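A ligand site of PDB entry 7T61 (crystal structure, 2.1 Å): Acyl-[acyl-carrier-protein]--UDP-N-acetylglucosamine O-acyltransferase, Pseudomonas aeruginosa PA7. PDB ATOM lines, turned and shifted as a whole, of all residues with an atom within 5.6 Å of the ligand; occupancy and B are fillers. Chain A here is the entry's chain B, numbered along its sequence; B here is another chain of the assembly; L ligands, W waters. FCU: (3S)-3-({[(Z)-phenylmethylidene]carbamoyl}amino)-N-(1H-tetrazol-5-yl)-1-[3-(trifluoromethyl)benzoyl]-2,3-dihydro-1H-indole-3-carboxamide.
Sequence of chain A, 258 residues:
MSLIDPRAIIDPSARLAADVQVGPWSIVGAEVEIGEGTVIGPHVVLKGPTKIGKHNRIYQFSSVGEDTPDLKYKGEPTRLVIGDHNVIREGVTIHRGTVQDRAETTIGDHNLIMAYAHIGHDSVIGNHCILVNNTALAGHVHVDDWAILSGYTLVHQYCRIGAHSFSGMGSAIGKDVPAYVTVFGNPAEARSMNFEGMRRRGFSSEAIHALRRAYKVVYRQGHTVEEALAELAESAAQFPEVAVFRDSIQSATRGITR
An oxygen (O28) of the ligand sits at hydrogen-bond distance from the backbone NH of Gln 157 (2.9 Å). The backbone NH of Gly 151 of chain B lies within hydrogen-bond range of an oxygen (O01) of the ligand (3.0 Å). N27 of the ligand sits at hydrogen-bond distance from NH1 of Arg 254, 3.3 Å away. O39 of the ligand sits at hydrogen-bond distance from NE2 of Gln 157 (2.8 Å).
A ring nitrogen (NE2) of His 121 sits at hydrogen-bond distance from the side-chain carboxylate of Asp 70 (2.9 Å). The side-chain hydroxyl (OG) of Ser 150 of chain B lies within hydrogen-bond range of the backbone carbonyl oxygen (O) of Ser 167 of chain B, at 2.7 Å. The backbone NH (N) of Asp 70 lies close to the side-chain hydroxyl (OG1) of Thr 68 (3.3 Å). The backbone carbonyl oxygen of Val 155 sits at hydrogen-bond distance from the backbone NH of Ala 138 (2.9 Å). The side-chain sulfur (SD) of Met 114 of chain B lies close to the side-chain amide oxygen (OD1) of Asn 133 of chain B (3.8 Å). O of His 118 is in hydrogen-bond range of N of Leu 137 (3.0 Å). The backbone NH of Val 155 is in hydrogen-bond range of the backbone carbonyl oxygen of Ala 136 (2.9 Å). The backbone carbonyl oxygen (O) of Asn 133 of chain B is in hydrogen-bond range of the backbone NH (N) of Tyr 152 of chain B (2.8 Å).
The backbone NH (N) of Ala 138 sits close to a fluorine (F11) of the ligand (3.2 Å). The side-chain amide oxygen (OD1) of Asn 133 of chain B sits close to a fluorine (F09) of the ligand, at 3.3 Å. Merely in contact with the ligand: Asp 70 (3.2 Å), Ser 150 of chain B (3.2 Å), His 118 (3.2 Å), Ala 136 (3.2 Å), Met 169 of chain B (3.3 Å), Val 132 of chain B (3.3 Å), His 121 (3.4 Å), Leu 137 (3.4 Å), Phe 166 of chain B (3.5 Å), Tyr 158 (3.5 Å), His 156 (3.6 Å), Thr 68 (3.7 Å) and Met 114 of chain B (3.8 Å). Hydrophobic or aromatic side chains within 4 Å of the ligand: His 118, His 121, Ala 136, Ala 138, His 156, Tyr 158, Met 114 of chain B, Val 132 of chain B, Phe 166 of chain B and Met 169 of chain B.
Water W2 lies within hydrogen-bond range of a nitrogen (N26) of the ligand and the guanidinium group (NH1) of Arg 254. Water W4 bridges the backbone NH of Met 169 of chain B and a ring nitrogen (NE2) of His 156. Water W1 lies within hydrogen-bond range of the backbone carbonyl oxygen (O) of Ala 138 (2.7 Å) and a ring nitrogen (NE2) of His 118 (2.8 Å).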
ATOM      1  N   THR A  68       9.007   1.451  -1.966  1.00  0.00           N
ATOM      2  CA  THR A  68       8.070   0.480  -2.585  1.00  0.00           C
ATOM      3  C   THR A  68       8.100  -0.816  -1.765  1.00  0.00           C
ATOM      4  O   THR A  68       9.165  -1.238  -1.312  1.00  0.00           O
ATOM      5  CB  THR A  68       8.447   0.146  -4.026  1.00  0.00           C
ATOM      6  OG1 THR A  68       7.404  -0.659  -4.593  1.00  0.00           O
ATOM      7  CG2 THR A  68       9.775  -0.577  -4.120  1.00  0.00           C
ATOM      8  N   PRO A  69       6.939  -1.483  -1.586  1.00  0.00           N
ATOM      9  CA  PRO A  69       6.934  -2.811  -0.967  1.00  0.00           C
ATOM     10  C   PRO A  69       7.459  -3.901  -1.911  1.00  0.00           C
ATOM     11  O   PRO A  69       7.668  -4.991  -1.442  1.00  0.00           O
ATOM     12  CB  PRO A  69       5.449  -3.011  -0.601  1.00  0.00           C
ATOM     13  CG  PRO A  69       4.680  -2.148  -1.579  1.00  0.00           C
ATOM     14  CD  PRO A  69       5.593  -0.994  -1.924  1.00  0.00           C
ATOM     15  N   ASP A  70       7.644  -3.599  -3.199  1.00  0.00           N
ATOM     16  CA  ASP A  70       8.158  -4.551  -4.221  1.00  0.00           C
ATOM     17  C   ASP A  70       9.345  -5.303  -3.614  1.00  0.00           C
ATOM     18  O   ASP A  70      10.341  -4.645  -3.207  1.00  0.00           O
ATOM     19  CB  ASP A  70       8.535  -3.830  -5.520  1.00  0.00           C
ATOM     20  CG  ASP A  70       8.819  -4.743  -6.708  1.00  0.00           C
ATOM     21  OD1 ASP A  70       9.342  -5.858  -6.503  1.00  0.00           O
ATOM     22  OD2 ASP A  70       8.517  -4.328  -7.857  1.00  0.00           O
ATOM     23  N   LEU A  71       9.267  -6.633  -3.580  1.00  0.00           N
ATOM     24  CA  LEU A  71      10.250  -7.515  -2.907  1.00  0.00           C
ATOM     25  C   LEU A  71      11.624  -7.381  -3.583  1.00  0.00           C
ATOM     26  O   LEU A  71      12.645  -7.617  -2.915  1.00  0.00           O
ATOM     27  CB  LEU A  71       9.725  -8.957  -2.928  1.00  0.00           C
ATOM     28  CG  LEU A  71       8.394  -9.164  -2.209  1.00  0.00           C
ATOM     29  CD1 LEU A  71       7.841 -10.560  -2.474  1.00  0.00           C
ATOM     30  CD2 LEU A  71       8.551  -8.937  -0.714  1.00  0.00           C
ATOM     31  N   HIS A 118      -2.391   6.392  -6.334  1.00  0.00           N
ATOM     32  CA  HIS A 118      -1.097   5.735  -6.029  1.00  0.00           C
ATOM     33  C   HIS A 118      -0.185   5.864  -7.244  1.00  0.00           C
ATOM     34  O   HIS A 118      -0.642   5.561  -8.350  1.00  0.00           O
ATOM     35  CB  HIS A 118      -1.314   4.274  -5.651  1.00  0.00           C
ATOM     36  CG  HIS A 118      -0.014   3.560  -5.567  1.00  0.00           C
ATOM     37  ND1 HIS A 118       0.922   3.890  -4.646  1.00  0.00           N
ATOM     38  CD2 HIS A 118       0.495   2.563  -6.311  1.00  0.00           C
ATOM     39  CE1 HIS A 118       1.973   3.102  -4.814  1.00  0.00           C
ATOM     40  NE2 HIS A 118       1.726   2.287  -5.821  1.00  0.00           N
ATOM     41  N   HIS A 121       6.725   2.811  -7.777  1.00  0.00           N
ATOM     42  CA  HIS A 121       8.185   2.982  -8.035  1.00  0.00           C
ATOM     43  C   HIS A 121       8.471   3.109  -9.521  1.00  0.00           C
ATOM     44  O   HIS A 121       7.945   2.277 -10.297  1.00  0.00           O
ATOM     45  CB  HIS A 121       8.970   1.816  -7.449  1.00  0.00           C
ATOM     46  CG  HIS A 121       8.682   0.477  -8.060  1.00  0.00           C
ATOM     47  ND1 HIS A 121       9.357   0.011  -9.178  1.00  0.00           N
ATOM     48  CD2 HIS A 121       7.843  -0.505  -7.671  1.00  0.00           C
ATOM     49  CE1 HIS A 121       8.935  -1.200  -9.451  1.00  0.00           C
ATOM     50  NE2 HIS A 121       8.000  -1.529  -8.561  1.00  0.00           N
ATOM     51  N   ALA A 136      -4.369   4.003  -9.699  1.00  0.00           N
ATOM     52  CA  ALA A 136      -3.194   3.256  -9.197  1.00  0.00           C
ATOM     53  C   ALA A 136      -2.278   2.892 -10.365  1.00  0.00           C
ATOM     54  O   ALA A 136      -2.751   2.232 -11.294  1.00  0.00           O
ATOM     55  CB  ALA A 136      -3.637   2.022  -8.438  1.00  0.00           C
ATOM     56  N   LEU A 137      -1.014   3.320 -10.292  1.00  0.00           N
ATOM     57  CA  LEU A 137       0.072   2.945 -11.242  1.00  0.00           C
ATOM     58  C   LEU A 137       1.013   1.993 -10.507  1.00  0.00           C
ATOM     59  O   LEU A 137       1.635   2.416  -9.510  1.00  0.00           O
ATOM     60  CB  LEU A 137       0.801   4.199 -11.729  1.00  0.00           C
ATOM     61  CG  LEU A 137      -0.046   5.434 -12.046  1.00  0.00           C
ATOM     62  CD1 LEU A 137       0.810   6.561 -12.584  1.00  0.00           C
ATOM     63  CD2 LEU A 137      -1.175   5.122 -13.029  1.00  0.00           C
ATOM     64  N   ALA A 138       1.077   0.729 -10.931  1.00  0.00           N
ATOM     65  CA  ALA A 138       1.791  -0.355 -10.209  1.00  0.00           C
ATOM     66  C   ALA A 138       3.290  -0.040 -10.101  1.00  0.00           C
ATOM     67  O   ALA A 138       3.867  -0.260  -9.030  1.00  0.00           O
ATOM     68  CB  ALA A 138       1.577  -1.674 -10.910  1.00  0.00           C
ATOM     69  N   GLY A 139       3.903   0.459 -11.176  1.00  0.00           N
ATOM     70  CA  GLY A 139       5.366   0.667 -11.238  1.00  0.00           C
ATOM     71  C   GLY A 139       5.852   0.804 -12.676  1.00  0.00           C
ATOM     72  O   GLY A 139       5.265   0.150 -13.566  1.00  0.00           O
ATOM     73  N   LEU A 154      -6.765   1.477 -13.033  1.00  0.00           N
ATOM     74  CA  LEU A 154      -5.670   0.586 -12.580  1.00  0.00           C
ATOM     75  C   LEU A 154      -4.695   0.402 -13.755  1.00  0.00           C
ATOM     76  O   LEU A 154      -5.185   0.120 -14.839  1.00  0.00           O
ATOM     77  CB  LEU A 154      -6.272  -0.756 -12.120  1.00  0.00           C
ATOM     78  CG  LEU A 154      -7.453  -0.659 -11.166  1.00  0.00           C
ATOM     79  CD1 LEU A 154      -7.920  -2.032 -10.743  1.00  0.00           C
ATOM     80  CD2 LEU A 154      -7.089   0.152  -9.947  1.00  0.00           C
ATOM     81  N   VAL A 155      -3.399   0.571 -13.536  1.00  0.00           N
ATOM     82  CA  VAL A 155      -2.336   0.410 -14.584  1.00  0.00           C
ATOM     83  C   VAL A 155      -1.266  -0.589 -14.117  1.00  0.00           C
ATOM     84  O   VAL A 155      -0.606  -0.331 -13.060  1.00  0.00           O
ATOM     85  CB  VAL A 155      -1.758   1.768 -15.019  1.00  0.00           C
ATOM     86  CG1 VAL A 155      -0.907   1.613 -16.271  1.00  0.00           C
ATOM     87  CG2 VAL A 155      -2.849   2.797 -15.262  1.00  0.00           C
ATOM     88  N   HIS A 156      -1.083  -1.628 -14.928  1.00  0.00           N
ATOM     89  CA  HIS A 156      -0.013  -2.626 -14.679  1.00  0.00           C
ATOM     90  C   HIS A 156       1.373  -2.015 -14.923  1.00  0.00           C
ATOM     91  O   HIS A 156       1.465  -0.988 -15.600  1.00  0.00           O
ATOM     92  CB  HIS A 156      -0.187  -3.839 -15.598  1.00  0.00           C
ATOM     93  CG  HIS A 156      -1.354  -4.726 -15.273  1.00  0.00           C
ATOM     94  ND1 HIS A 156      -2.641  -4.387 -15.594  1.00  0.00           N
ATOM     95  CD2 HIS A 156      -1.405  -5.935 -14.687  1.00  0.00           C
ATOM     96  CE1 HIS A 156      -3.454  -5.357 -15.200  1.00  0.00           C
ATOM     97  NE2 HIS A 156      -2.714  -6.310 -14.643  1.00  0.00           N
ATOM     98  N   GLN A 157       2.405  -2.681 -14.426  1.00  0.00           N
ATOM     99  CA  GLN A 157       3.814  -2.214 -14.566  1.00  0.00           C
ATOM    100  C   GLN A 157       4.167  -2.090 -16.047  1.00  0.00           C
ATOM    101  O   GLN A 157       3.693  -2.907 -16.853  1.00  0.00           O
ATOM    102  CB  GLN A 157       4.812  -3.153 -13.882  1.00  0.00           C
ATOM    103  CG  GLN A 157       4.801  -3.043 -12.373  1.00  0.00           C
ATOM    104  CD  GLN A 157       6.105  -3.479 -11.745  1.00  0.00           C
ATOM    105  OE1 GLN A 157       6.819  -2.686 -11.147  1.00  0.00           O
ATOM    106  NE2 GLN A 157       6.434  -4.753 -11.880  1.00  0.00           N
ATOM    107  N   TYR A 158       5.011  -1.093 -16.352  1.00  0.00           N
ATOM    108  CA  TYR A 158       5.711  -0.907 -17.651  1.00  0.00           C
ATOM    109  C   TYR A 158       4.736  -0.423 -18.733  1.00  0.00           C
ATOM    110  O   TYR A 158       5.161  -0.234 -19.858  1.00  0.00           O
ATOM    111  CB  TYR A 158       6.411  -2.207 -18.082  1.00  0.00           C
ATOM    112  CG  TYR A 158       7.534  -2.620 -17.174  1.00  0.00           C
ATOM    113  CD1 TYR A 158       8.744  -1.928 -17.170  1.00  0.00           C
ATOM    114  CD2 TYR A 158       7.403  -3.682 -16.318  1.00  0.00           C
ATOM    115  CE1 TYR A 158       9.776  -2.289 -16.329  1.00  0.00           C
ATOM    116  CE2 TYR A 158       8.434  -4.067 -15.474  1.00  0.00           C
ATOM    117  CZ  TYR A 158       9.626  -3.366 -15.476  1.00  0.00           C
ATOM    118  OH  TYR A 158      10.655  -3.725 -14.659  1.00  0.00           O
ATOM    119  N   ARG A 254       4.334  -3.477 -24.074  1.00  0.00           N
ATOM    120  CA  ARG A 254       3.322  -4.466 -23.595  1.00  0.00           C
ATOM    121  C   ARG A 254       2.258  -4.687 -24.673  1.00  0.00           C
ATOM    122  O   ARG A 254       1.226  -5.325 -24.380  1.00  0.00           O
ATOM    123  CB  ARG A 254       2.748  -3.986 -22.253  1.00  0.00           C
ATOM    124  CG  ARG A 254       3.653  -4.318 -21.076  1.00  0.00           C
ATOM    125  CD  ARG A 254       3.082  -3.894 -19.759  1.00  0.00           C
ATOM    126  NE  ARG A 254       1.885  -4.656 -19.436  1.00  0.00           N
ATOM    127  CZ  ARG A 254       1.859  -5.806 -18.757  1.00  0.00           C
ATOM    128  NH1 ARG A 254       2.980  -6.345 -18.306  1.00  0.00           N
ATOM    129  NH2 ARG A 254       0.694  -6.411 -18.544  1.00  0.00           N
ATOM    130  N   MET B 114      -0.774  -4.454   1.329  1.00  0.00           N
ATOM    131  CA  MET B 114      -0.318  -3.205   0.665  1.00  0.00           C
ATOM    132  C   MET B 114      -1.372  -2.123   0.909  1.00  0.00           C
ATOM    133  O   MET B 114      -2.427  -2.438   1.501  1.00  0.00           O
ATOM    134  CB  MET B 114      -0.067  -3.430  -0.831  1.00  0.00           C
ATOM    135  CG  MET B 114       1.017  -4.491  -1.097  1.00  0.00           C
ATOM    136  SD  MET B 114       1.698  -4.380  -2.756  1.00  0.00           S
ATOM    137  CE  MET B 114       2.376  -6.016  -2.953  1.00  0.00           C
ATOM    138  N   VAL B 132      -2.540  -6.948  -2.624  1.00  0.00           N
ATOM    139  CA  VAL B 132      -2.042  -5.733  -3.326  1.00  0.00           C
ATOM    140  C   VAL B 132      -3.008  -4.592  -3.009  1.00  0.00           C
ATOM    141  O   VAL B 132      -4.116  -4.859  -2.467  1.00  0.00           O
ATOM    142  CB  VAL B 132      -1.838  -6.009  -4.828  1.00  0.00           C
ATOM    143  CG1 VAL B 132      -1.411  -4.791  -5.636  1.00  0.00           C
ATOM    144  CG2 VAL B 132      -0.842  -7.138  -5.036  1.00  0.00           C
ATOM    145  N   ASN B 133      -2.580  -3.354  -3.266  1.00  0.00           N
ATOM    146  CA  ASN B 133      -3.324  -2.107  -2.967  1.00  0.00           C
ATOM    147  C   ASN B 133      -4.843  -2.308  -3.084  1.00  0.00           C
ATOM    148  O   ASN B 133      -5.311  -2.761  -4.140  1.00  0.00           O
ATOM    149  CB  ASN B 133      -2.875  -0.967  -3.892  1.00  0.00           C
ATOM    150  CG  ASN B 133      -1.406  -0.618  -3.711  1.00  0.00           C
ATOM    151  OD1 ASN B 133      -0.541  -1.501  -3.774  1.00  0.00           O
ATOM    152  ND2 ASN B 133      -1.110   0.659  -3.524  1.00  0.00           N
ATOM    153  N   SER B 150      -4.356  -9.418  -6.524  1.00  0.00           N
ATOM    154  CA  SER B 150      -3.788  -8.276  -7.273  1.00  0.00           C
ATOM    155  C   SER B 150      -4.568  -7.024  -6.887  1.00  0.00           C
ATOM    156  O   SER B 150      -5.578  -7.166  -6.161  1.00  0.00           O
ATOM    157  CB  SER B 150      -3.799  -8.531  -8.760  1.00  0.00           C
ATOM    158  OG  SER B 150      -2.827  -9.499  -9.116  1.00  0.00           O
ATOM    159  N   GLY B 151      -4.110  -5.841  -7.331  1.00  0.00           N
ATOM    160  CA  GLY B 151      -4.658  -4.551  -6.878  1.00  0.00           C
ATOM    161  C   GLY B 151      -6.179  -4.536  -7.013  1.00  0.00           C
ATOM    162  O   GLY B 151      -6.658  -4.954  -8.089  1.00  0.00           O
ATOM    163  N   TYR B 152      -6.891  -4.049  -6.000  1.00  0.00           N
ATOM    164  CA  TYR B 152      -8.345  -3.750  -6.040  1.00  0.00           C
ATOM    165  C   TYR B 152      -9.168  -5.038  -6.271  1.00  0.00           C
ATOM    166  O   TYR B 152     -10.239  -5.004  -6.884  1.00  0.00           O
ATOM    167  CB  TYR B 152      -8.627  -2.672  -7.112  1.00  0.00           C
ATOM    168  CG  TYR B 152      -8.142  -1.283  -6.753  1.00  0.00           C
ATOM    169  CD1 TYR B 152      -6.793  -0.991  -6.727  1.00  0.00           C
ATOM    170  CD2 TYR B 152      -9.032  -0.264  -6.468  1.00  0.00           C
ATOM    171  CE1 TYR B 152      -6.321   0.279  -6.405  1.00  0.00           C
ATOM    172  CE2 TYR B 152      -8.574   1.008  -6.136  1.00  0.00           C
ATOM    173  CZ  TYR B 152      -7.220   1.278  -6.121  1.00  0.00           C
ATOM    174  OH  TYR B 152      -6.771   2.516  -5.816  1.00  0.00           O
ATOM    175  N   PHE B 166      -4.318 -17.007  -7.378  1.00  0.00           N
ATOM    176  CA  PHE B 166      -3.977 -15.679  -7.919  1.00  0.00           C
ATOM    177  C   PHE B 166      -5.228 -15.016  -8.501  1.00  0.00           C
ATOM    178  O   PHE B 166      -5.940 -15.655  -9.299  1.00  0.00           O
ATOM    179  CB  PHE B 166      -2.869 -15.817  -8.966  1.00  0.00           C
ATOM    180  CG  PHE B 166      -2.503 -14.532  -9.654  1.00  0.00           C
ATOM    181  CD1 PHE B 166      -1.558 -13.658  -9.107  1.00  0.00           C
ATOM    182  CD2 PHE B 166      -3.092 -14.191 -10.861  1.00  0.00           C
ATOM    183  CE1 PHE B 166      -1.213 -12.487  -9.765  1.00  0.00           C
ATOM    184  CE2 PHE B 166      -2.757 -13.007 -11.504  1.00  0.00           C
ATOM    185  CZ  PHE B 166      -1.827 -12.156 -10.945  1.00  0.00           C
ATOM    186  N   SER B 167      -5.469 -13.767  -8.131  1.00  0.00           N
ATOM    187  CA  SER B 167      -6.538 -12.939  -8.766  1.00  0.00           C
ATOM    188  C   SER B 167      -5.907 -11.831  -9.621  1.00  0.00           C
ATOM    189  O   SER B 167      -4.903 -11.252  -9.181  1.00  0.00           O
ATOM    190  CB  SER B 167      -7.459 -12.388  -7.725  1.00  0.00           C
ATOM    191  OG  SER B 167      -6.836 -11.323  -7.031  1.00  0.00           O
ATOM    192  N   GLY B 168      -6.497 -11.522 -10.764  1.00  0.00           N
ATOM    193  CA  GLY B 168      -6.080 -10.421 -11.656  1.00  0.00           C
ATOM    194  C   GLY B 168      -6.546  -9.111 -11.063  1.00  0.00           C
ATOM    195  O   GLY B 168      -7.458  -9.120 -10.214  1.00  0.00           O
ATOM    196  N   MET B 169      -5.965  -7.989 -11.515  1.00  0.00           N
ATOM    197  CA  MET B 169      -6.305  -6.650 -10.981  1.00  0.00           C
ATOM    198  C   MET B 169      -7.817  -6.404 -11.142  1.00  0.00           C
ATOM    199  O   MET B 169      -8.393  -6.819 -12.165  1.00  0.00           O
ATOM    200  CB  MET B 169      -5.501  -5.558 -11.673  1.00  0.00           C
ATOM    201  CG  MET B 169      -4.202  -5.309 -10.959  1.00  0.00           C
ATOM    202  SD  MET B 169      -3.767  -3.607 -10.938  1.00  0.00           S
ATOM    203  CE  MET B 169      -3.648  -3.289 -12.695  1.00  0.00           C
ATOM    204  N   PHE B 184      -9.868 -13.853 -12.976  1.00  0.00           N
ATOM    205  CA  PHE B 184      -9.859 -12.493 -13.555  1.00  0.00           C
ATOM    206  C   PHE B 184     -11.285 -11.974 -13.741  1.00  0.00           C
ATOM    207  O   PHE B 184     -12.161 -12.773 -14.087  1.00  0.00           O
ATOM    208  CB  PHE B 184      -9.162 -12.509 -14.914  1.00  0.00           C
ATOM    209  CG  PHE B 184      -7.745 -12.985 -14.856  1.00  0.00           C
ATOM    210  CD1 PHE B 184      -7.458 -14.341 -14.878  1.00  0.00           C
ATOM    211  CD2 PHE B 184      -6.697 -12.085 -14.744  1.00  0.00           C
ATOM    212  CE1 PHE B 184      -6.135 -14.786 -14.806  1.00  0.00           C
ATOM    213  CE2 PHE B 184      -5.387 -12.534 -14.671  1.00  0.00           C
ATOM    214  CZ  PHE B 184      -5.109 -13.886 -14.695  1.00  0.00           C
HETATM  215  O01 FCU L   1      -1.649  -6.136  -9.007  1.00  0.00           O
HETATM  216  C02 FCU L   1      -0.706  -5.559  -9.451  1.00  0.00           C
HETATM  217  C03 FCU L   1      -0.159  -4.362  -8.707  1.00  0.00           C
HETATM  218  C04 FCU L   1       1.084  -4.453  -8.033  1.00  0.00           C
HETATM  219  C05 FCU L   1       1.546  -3.339  -7.303  1.00  0.00           C
HETATM  220  C06 FCU L   1       0.770  -2.176  -7.222  1.00  0.00           C
HETATM  221  C07 FCU L   1      -0.481  -2.141  -7.888  1.00  0.00           C
HETATM  222  C08 FCU L   1      -1.380  -0.905  -7.851  1.00  0.00           C
HETATM  223  F09 FCU L   1      -1.048  -0.211  -6.716  1.00  0.00           F
HETATM  224  F10 FCU L   1      -2.657  -1.350  -7.800  1.00  0.00           F
HETATM  225  F11 FCU L   1      -1.259  -0.066  -8.961  1.00  0.00           F
HETATM  226  C12 FCU L   1      -0.942  -3.226  -8.612  1.00  0.00           C
HETATM  227  N13 FCU L   1      -0.084  -6.025 -10.662  1.00  0.00           N
HETATM  228  C14 FCU L   1      -0.466  -7.243 -11.482  1.00  0.00           C
HETATM  229  C15 FCU L   1       0.712  -7.652 -12.111  1.00  0.00           C
HETATM  230  C16 FCU L   1       0.723  -8.778 -12.959  1.00  0.00           C
HETATM  231  C17 FCU L   1      -0.481  -9.493 -13.167  1.00  0.00           C
HETATM  232  C18 FCU L   1      -1.656  -9.091 -12.522  1.00  0.00           C
HETATM  233  C19 FCU L   1      -1.668  -7.984 -11.664  1.00  0.00           C
HETATM  234  C20 FCU L   1       1.811  -6.660 -11.717  1.00  0.00           C
HETATM  235  C21 FCU L   1       2.760  -6.396 -12.904  1.00  0.00           C
HETATM  236  N22 FCU L   1       3.863  -7.324 -13.095  1.00  0.00           N
HETATM  237  C23 FCU L   1       4.803  -7.137 -14.193  1.00  0.00           C
HETATM  238  N24 FCU L   1       6.112  -7.345 -14.140  1.00  0.00           N
HETATM  239  N25 FCU L   1       6.624  -7.062 -15.350  1.00  0.00           N
HETATM  240  N26 FCU L   1       5.613  -6.679 -16.147  1.00  0.00           N
HETATM  241  N27 FCU L   1       4.496  -6.742 -15.433  1.00  0.00           N
HETATM  242  O28 FCU L   1       2.613  -5.478 -13.664  1.00  0.00           O
HETATM  243  N29 FCU L   1       2.574  -7.214 -10.591  1.00  0.00           N
HETATM  244  C30 FCU L   1       3.718  -6.508 -10.058  1.00  0.00           C
HETATM  245  N31 FCU L   1       4.438  -7.097  -8.926  1.00  0.00           N
HETATM  246  C32 FCU L   1       5.615  -6.382  -8.409  1.00  0.00           C
HETATM  247  C33 FCU L   1       5.311  -5.175  -7.535  1.00  0.00           C
HETATM  248  C34 FCU L   1       5.380  -3.891  -8.059  1.00  0.00           C
HETATM  249  C35 FCU L   1       5.125  -2.767  -7.252  1.00  0.00           C
HETATM  250  C36 FCU L   1       4.809  -2.926  -5.911  1.00  0.00           C
HETATM  251  C37 FCU L   1       4.727  -4.213  -5.386  1.00  0.00           C
HETATM  252  C38 FCU L   1       4.985  -5.349  -6.186  1.00  0.00           C
HETATM  253  O39 FCU L   1       4.046  -5.435 -10.525  1.00  0.00           O
HETATM  254  C40 FCU L   1       1.083  -5.429 -11.306  1.00  0.00           C
HETATM  255  O   HOH W   1       3.286  -0.016  -6.420  1.00  0.00           O
HETATM  256  O   HOH W   2       6.218  -5.927 -19.234  1.00  0.00           O
HETATM  257  O   HOH W   3      -2.728 -10.412 -15.495  1.00  0.00           O
HETATM  258  O   HOH W   4      -4.550  -8.546 -14.028  1.00  0.00           O
HETATM  259  O   HOH W   5       4.892  -9.745 -12.302  1.00  0.00           O
